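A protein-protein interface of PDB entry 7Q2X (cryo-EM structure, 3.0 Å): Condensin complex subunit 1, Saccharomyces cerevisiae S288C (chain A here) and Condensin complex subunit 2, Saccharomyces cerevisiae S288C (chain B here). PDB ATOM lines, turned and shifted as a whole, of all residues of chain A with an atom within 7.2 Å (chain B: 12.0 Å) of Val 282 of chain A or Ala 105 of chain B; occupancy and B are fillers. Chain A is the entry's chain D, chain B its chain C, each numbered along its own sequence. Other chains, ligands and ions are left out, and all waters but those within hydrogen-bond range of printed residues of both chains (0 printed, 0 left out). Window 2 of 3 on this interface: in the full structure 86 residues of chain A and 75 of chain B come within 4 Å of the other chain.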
ATOM      1  N   GLU A 277      12.046  -2.906  38.569  1.00  0.00           N
ATOM      2  CA  GLU A 277      11.399  -2.347  37.386  1.00  0.00           C
ATOM      3  C   GLU A 277      12.238  -1.233  36.773  1.00  0.00           C
ATOM      4  O   GLU A 277      12.311  -1.105  35.546  1.00  0.00           O
ATOM      5  CB  GLU A 277      10.004  -1.833  37.738  1.00  0.00           C
ATOM      6  CG  GLU A 277       8.952  -2.921  37.847  1.00  0.00           C
ATOM      7  CD  GLU A 277       7.542  -2.368  37.820  1.00  0.00           C
ATOM      8  OE1 GLU A 277       6.973  -2.239  36.716  1.00  0.00           O
ATOM      9  OE2 GLU A 277       7.006  -2.053  38.901  1.00  0.00           O
ATOM     10  N   ILE A 278      12.871  -0.412  37.614  1.00  0.00           N
ATOM     11  CA  ILE A 278      13.767   0.627  37.108  1.00  0.00           C
ATOM     12  C   ILE A 278      14.930  -0.001  36.355  1.00  0.00           C
ATOM     13  O   ILE A 278      15.329   0.475  35.285  1.00  0.00           O
ATOM     14  CB  ILE A 278      14.259   1.521  38.262  1.00  0.00           C
ATOM     15  CG1 ILE A 278      13.092   2.275  38.898  1.00  0.00           C
ATOM     16  CG2 ILE A 278      15.320   2.493  37.771  1.00  0.00           C
ATOM     17  CD1 ILE A 278      12.322   3.127  37.929  1.00  0.00           C
ATOM     18  N   SER A 279      15.495  -1.079  36.904  1.00  0.00           N
ATOM     19  CA  SER A 279      16.602  -1.758  36.239  1.00  0.00           C
ATOM     20  C   SER A 279      16.172  -2.329  34.893  1.00  0.00           C
ATOM     21  O   SER A 279      16.925  -2.261  33.914  1.00  0.00           O
ATOM     22  CB  SER A 279      17.153  -2.864  37.138  1.00  0.00           C
ATOM     23  OG  SER A 279      16.159  -3.833  37.414  1.00  0.00           O
ATOM     24  N   THR A 280      14.971  -2.898  34.823  1.00  0.00           N
ATOM     25  CA  THR A 280      14.476  -3.491  33.587  1.00  0.00           C
ATOM     26  C   THR A 280      13.747  -2.496  32.690  1.00  0.00           C
ATOM     27  O   THR A 280      13.316  -2.874  31.595  1.00  0.00           O
ATOM     28  CB  THR A 280      13.548  -4.672  33.901  1.00  0.00           C
ATOM     29  OG1 THR A 280      13.401  -5.489  32.733  1.00  0.00           O
ATOM     30  CG2 THR A 280      12.177  -4.176  34.336  1.00  0.00           C
ATOM     31  N   ARG A 281      13.602  -1.244  33.116  1.00  0.00           N
ATOM     32  CA  ARG A 281      12.881  -0.258  32.321  1.00  0.00           C
ATOM     33  C   ARG A 281      13.690   0.146  31.092  1.00  0.00           C
ATOM     34  O   ARG A 281      14.921   0.228  31.127  1.00  0.00           O
ATOM     35  CB  ARG A 281      12.558   0.975  33.169  1.00  0.00           C
ATOM     36  CG  ARG A 281      11.904   2.116  32.406  1.00  0.00           C
ATOM     37  CD  ARG A 281      10.823   2.795  33.229  1.00  0.00           C
ATOM     38  NE  ARG A 281       9.895   3.544  32.389  1.00  0.00           N
ATOM     39  CZ  ARG A 281       8.778   3.044  31.878  1.00  0.00           C
ATOM     40  NH1 ARG A 281       8.406   1.798  32.120  1.00  0.00           N
ATOM     41  NH2 ARG A 281       8.016   3.813  31.107  1.00  0.00           N
ATOM     42  N   VAL A 282      12.981   0.399  29.994  1.00  0.00           N
ATOM     43  CA  VAL A 282      13.578   0.825  28.734  1.00  0.00           C
ATOM     44  C   VAL A 282      12.990   2.181  28.359  1.00  0.00           C
ATOM     45  O   VAL A 282      11.798   2.429  28.577  1.00  0.00           O
ATOM     46  CB  VAL A 282      13.353  -0.215  27.618  1.00  0.00           C
ATOM     47  CG1 VAL A 282      11.869  -0.391  27.325  1.00  0.00           C
ATOM     48  CG2 VAL A 282      14.112   0.175  26.358  1.00  0.00           C
ATOM     49  N   PHE A 283      13.832   3.063  27.822  1.00  0.00           N
ATOM     50  CA  PHE A 283      13.434   4.408  27.434  1.00  0.00           C
ATOM     51  C   PHE A 283      13.685   4.621  25.949  1.00  0.00           C
ATOM     52  O   PHE A 283      14.626   4.060  25.380  1.00  0.00           O
ATOM     53  CB  PHE A 283      14.194   5.469  28.240  1.00  0.00           C
ATOM     54  CG  PHE A 283      14.147   5.253  29.725  1.00  0.00           C
ATOM     55  CD1 PHE A 283      13.054   5.674  30.463  1.00  0.00           C
ATOM     56  CD2 PHE A 283      15.192   4.627  30.382  1.00  0.00           C
ATOM     57  CE1 PHE A 283      13.006   5.481  31.829  1.00  0.00           C
ATOM     58  CE2 PHE A 283      15.147   4.427  31.748  1.00  0.00           C
ATOM     59  CZ  PHE A 283      14.054   4.857  32.472  1.00  0.00           C
ATOM     60  N   ASN A 284      12.835   5.435  25.327  1.00  0.00           N
ATOM     61  CA  ASN A 284      13.002   5.768  23.921  1.00  0.00           C
ATOM     62  C   ASN A 284      14.108   6.803  23.742  1.00  0.00           C
ATOM     63  O   ASN A 284      14.555   7.453  24.692  1.00  0.00           O
ATOM     64  CB  ASN A 284      11.690   6.291  23.336  1.00  0.00           C
ATOM     65  CG  ASN A 284      10.590   5.251  23.353  1.00  0.00           C
ATOM     66  OD1 ASN A 284       9.600   5.393  24.070  1.00  0.00           O
ATOM     67  ND2 ASN A 284      10.756   4.199  22.561  1.00  0.00           N
ATOM     68  N   ASP A 287      12.393  10.909  24.220  1.00  0.00           N
ATOM     69  CA  ASP A 287      12.025  11.499  25.499  1.00  0.00           C
ATOM     70  C   ASP A 287      13.223  11.532  26.438  1.00  0.00           C
ATOM     71  O   ASP A 287      14.025  10.595  26.480  1.00  0.00           O
ATOM     72  CB  ASP A 287      10.874  10.722  26.141  1.00  0.00           C
ATOM     73  CG  ASP A 287      11.293   9.351  26.628  1.00  0.00           C
ATOM     74  OD1 ASP A 287      11.982   8.634  25.871  1.00  0.00           O
ATOM     75  OD2 ASP A 287      10.934   8.987  27.768  1.00  0.00           O
ATOM     76  N   LEU A 319      21.944  -1.407  35.040  1.00  0.00           N
ATOM     77  CA  LEU A 319      21.415  -0.252  34.325  1.00  0.00           C
ATOM     78  C   LEU A 319      22.510   0.727  33.920  1.00  0.00           C
ATOM     79  O   LEU A 319      22.284   1.567  33.042  1.00  0.00           O
ATOM     80  CB  LEU A 319      20.367   0.457  35.189  1.00  0.00           C
ATOM     81  CG  LEU A 319      19.559   1.603  34.577  1.00  0.00           C
ATOM     82  CD1 LEU A 319      18.723   1.106  33.409  1.00  0.00           C
ATOM     83  CD2 LEU A 319      18.683   2.262  35.630  1.00  0.00           C
ATOM     84  N   ASN A 322      23.564   1.517  30.215  1.00  0.00           N
ATOM     85  CA  ASN A 322      22.737   2.315  29.326  1.00  0.00           C
ATOM     86  C   ASN A 322      23.492   3.559  28.862  1.00  0.00           C
ATOM     87  O   ASN A 322      24.354   4.097  29.561  1.00  0.00           O
ATOM     88  CB  ASN A 322      21.437   2.716  30.028  1.00  0.00           C
ATOM     89  CG  ASN A 322      20.438   3.370  29.089  1.00  0.00           C
ATOM     90  OD1 ASN A 322      20.709   3.561  27.904  1.00  0.00           O
ATOM     91  ND2 ASN A 322      19.273   3.719  29.621  1.00  0.00           N
ATOM     92  N   GLU B  96       5.309  14.833  24.506  1.00  0.00           N
ATOM     93  CA  GLU B  96       4.153  14.033  24.901  1.00  0.00           C
ATOM     94  C   GLU B  96       4.149  12.691  24.179  1.00  0.00           C
ATOM     95  O   GLU B  96       3.861  11.649  24.786  1.00  0.00           O
ATOM     96  CB  GLU B  96       2.857  14.792  24.611  1.00  0.00           C
ATOM     97  CG  GLU B  96       2.565  16.003  25.499  1.00  0.00           C
ATOM     98  CD  GLU B  96       2.636  15.702  26.984  1.00  0.00           C
ATOM     99  OE1 GLU B  96       1.568  15.498  27.600  1.00  0.00           O
ATOM    100  OE2 GLU B  96       3.750  15.707  27.545  1.00  0.00           O
ATOM    101  N   THR B  97       4.465  12.698  22.882  1.00  0.00           N
ATOM    102  CA  THR B  97       4.558  11.450  22.134  1.00  0.00           C
ATOM    103  C   THR B  97       5.663  10.562  22.689  1.00  0.00           C
ATOM    104  O   THR B  97       5.494   9.341  22.794  1.00  0.00           O
ATOM    105  CB  THR B  97       4.797  11.740  20.651  1.00  0.00           C
ATOM    106  OG1 THR B  97       3.729  12.547  20.142  1.00  0.00           O
ATOM    107  CG2 THR B  97       4.862  10.444  19.857  1.00  0.00           C
ATOM    108  N   GLY B  98       6.802  11.156  23.047  1.00  0.00           N
ATOM    109  CA  GLY B  98       7.867  10.380  23.661  1.00  0.00           C
ATOM    110  C   GLY B  98       7.450   9.749  24.976  1.00  0.00           C
ATOM    111  O   GLY B  98       7.751   8.580  25.239  1.00  0.00           O
ATOM    112  N   LYS B  99       6.747  10.511  25.819  1.00  0.00           N
ATOM    113  CA  LYS B  99       6.250   9.957  27.076  1.00  0.00           C
ATOM    114  C   LYS B  99       5.282   8.809  26.827  1.00  0.00           C
ATOM    115  O   LYS B  99       5.336   7.780  27.511  1.00  0.00           O
ATOM    116  CB  LYS B  99       5.565  11.040  27.911  1.00  0.00           C
ATOM    117  CG  LYS B  99       6.467  12.149  28.415  1.00  0.00           C
ATOM    118  CD  LYS B  99       5.705  13.463  28.444  1.00  0.00           C
ATOM    119  CE  LYS B  99       6.476  14.563  29.149  1.00  0.00           C
ATOM    120  NZ  LYS B  99       6.048  14.718  30.567  1.00  0.00           N
ATOM    121  N   LEU B 100       4.377   8.970  25.857  1.00  0.00           N
ATOM    122  CA  LEU B 100       3.407   7.917  25.572  1.00  0.00           C
ATOM    123  C   LEU B 100       4.097   6.662  25.047  1.00  0.00           C
ATOM    124  O   LEU B 100       3.731   5.539  25.413  1.00  0.00           O
ATOM    125  CB  LEU B 100       2.361   8.423  24.579  1.00  0.00           C
ATOM    126  CG  LEU B 100       1.051   7.633  24.526  1.00  0.00           C
ATOM    127  CD1 LEU B 100       0.583   7.277  25.926  1.00  0.00           C
ATOM    128  CD2 LEU B 100      -0.019   8.427  23.799  1.00  0.00           C
ATOM    129  N   LEU B 101       5.103   6.835  24.185  1.00  0.00           N
ATOM    130  CA  LEU B 101       5.852   5.687  23.682  1.00  0.00           C
ATOM    131  C   LEU B 101       6.601   4.982  24.805  1.00  0.00           C
ATOM    132  O   LEU B 101       6.653   3.747  24.846  1.00  0.00           O
ATOM    133  CB  LEU B 101       6.825   6.128  22.590  1.00  0.00           C
ATOM    134  CG  LEU B 101       6.219   6.627  21.279  1.00  0.00           C
ATOM    135  CD1 LEU B 101       7.199   7.552  20.580  1.00  0.00           C
ATOM    136  CD2 LEU B 101       5.839   5.463  20.381  1.00  0.00           C
ATOM    137  N   SER B 102       7.198   5.749  25.720  1.00  0.00           N
ATOM    138  CA  SER B 102       7.872   5.139  26.862  1.00  0.00           C
ATOM    139  C   SER B 102       6.886   4.379  27.739  1.00  0.00           C
ATOM    140  O   SER B 102       7.203   3.300  28.253  1.00  0.00           O
ATOM    141  CB  SER B 102       8.603   6.207  27.674  1.00  0.00           C
ATOM    142  OG  SER B 102       9.657   6.783  26.923  1.00  0.00           O
ATOM    143  N   GLY B 103       5.687   4.932  27.927  1.00  0.00           N
ATOM    144  CA  GLY B 103       4.670   4.226  28.689  1.00  0.00           C
ATOM    145  C   GLY B 103       4.215   2.947  28.010  1.00  0.00           C
ATOM    146  O   GLY B 103       3.917   1.952  28.678  1.00  0.00           O
ATOM    147  N   LEU B 104       4.155   2.954  26.681  1.00  0.00           N
ATOM    148  CA  LEU B 104       3.767   1.780  25.910  1.00  0.00           C
ATOM    149  C   LEU B 104       4.951   0.905  25.519  1.00  0.00           C
ATOM    150  O   LEU B 104       4.759  -0.093  24.818  1.00  0.00           O
ATOM    151  CB  LEU B 104       3.007   2.202  24.649  1.00  0.00           C
ATOM    152  CG  LEU B 104       1.648   2.867  24.865  1.00  0.00           C
ATOM    153  CD1 LEU B 104       1.076   3.356  23.547  1.00  0.00           C
ATOM    154  CD2 LEU B 104       0.692   1.894  25.537  1.00  0.00           C
ATOM    155  N   ALA B 105       6.166   1.253  25.948  1.00  0.00           N
ATOM    156  CA  ALA B 105       7.339   0.452  25.620  1.00  0.00           C
ATOM    157  C   ALA B 105       7.346  -0.902  26.314  1.00  0.00           C
ATOM    158  O   ALA B 105       8.053  -1.806  25.859  1.00  0.00           O
ATOM    159  CB  ALA B 105       8.614   1.219  25.975  1.00  0.00           C
ATOM    160  N   GLN B 106       6.587  -1.067  27.393  1.00  0.00           N
ATOM    161  CA  GLN B 106       6.527  -2.340  28.101  1.00  0.00           C
ATOM    162  C   GLN B 106       5.089  -2.836  28.215  1.00  0.00           C
ATOM    163  O   GLN B 106       4.839  -3.935  28.709  1.00  0.00           O
ATOM    164  CB  GLN B 106       7.150  -2.216  29.493  1.00  0.00           C
ATOM    165  CG  GLN B 106       8.553  -1.633  29.496  1.00  0.00           C
ATOM    166  CD  GLN B 106       8.914  -0.994  30.822  1.00  0.00           C
ATOM    167  OE1 GLN B 106       9.845  -0.194  30.905  1.00  0.00           O
ATOM    168  NE2 GLN B 106       8.177  -1.346  31.869  1.00  0.00           N
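Val 282 of chain A touches just these residues of chain B: Ala 105 and Gln 106. Of chain A, only Val 282 (3.9 Å) comes within 4 Å of Ala 105 of chain B. No residue of chain B comes within 4 Å of Thr 280 of chain A. Of chain B, only Ser 102 (3.0 Å) and Gln 106 (2.7 Å) come within 4 Å of Arg 281 of chain A. No residue of chain B comes within 4 Å of Phe 283 of chain A. Asn 284 of chain A touches just these residues of chain B: Gly 98, Leu 101 and Ser 102. Printed residues of chain A within 4 Å of Ser 102 of chain B: Arg 281, Asn 284 and Asp 287. Of the printed residues of chain A, Gln 106 of chain B touches Arg 281 and Val 282. Printed residues of chain A within 4 Å of Leu 101 of chain B: Asn 284. Printed residues of chain B within 4 Å of Asp 287 of chain A: Gly 98 (3.7 Å) and Ser 102 (2.7 Å). Of the printed residues of chain A, Gly 98 of chain B touches Asn 284 (3.9 Å) and Asp 287 (3.7 Å).
The backbone carbonyl oxygen (O) of Leu 101 of chain B lies close to the side-chain amide oxygen (OD1) of Asn 284 of chain A, at 3.5 Å. O of Ser 102 of chain B lies within hydrogen-bond range of NH2 of Arg 281 of chain A (3.0 Å). N of Ser 102 of chain B sits at hydrogen-bond distance from OD1 of Asn 284 of chain A. The side-chain carboxylate (OD2) of Asp 287 of chain A lies within hydrogen-bond range of the side-chain hydroxyl (OG) of Ser 102 of chain B, at 2.7 Å. NH1 of Arg 281 of chain A lies within hydrogen-bond range of OE1 of Gln 106 of chain B (2.7 Å). The side-chain amide oxygen (OE1) of Gln 106 of chain B sits at hydrogen-bond distance from the backbone NH (N) of Val 282 of chain A.
Hydrophobic or aromatic side chains of chain B that line the printed part of chain A: Leu 101 and Ala 105. Along chain B the printed residues that touch a printed residue of chain A span positions 98 to 106. Printed residues of chain A that touch a printed residue of chain B: Arg 281, Val 282, Asn 284 and Asp 287. Hydrophobic or aromatic side chains of chain A within 4 Å of the printed part of chain B: Val 282. Among the printed residues, 9 pairs touch across the chains. Among the printed residues, no Asp or Glu carboxylate lies within 4 Å of a Lys or Arg side-chain nitrogen of the other chain.
Among the printed residues, merely in contact across the chains: Val 282 of chain A with Ala 105 of chain B (3.9 Å), Asn 284 of chain A with Gly 98 of chain B (3.9 Å) and Asp 287 of chain A with Gly 98 of chain B (3.7 Å).
O of Gly 98 of chain B sits at hydrogen-bond distance from OG of Ser 102 of chain B (3.1 Å). The backbone NH (N) of Asn 284 of chain A lies within hydrogen-bond range of the side-chain carboxylate (OD1) of Asp 287 of chain A, 3.4 Å away.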
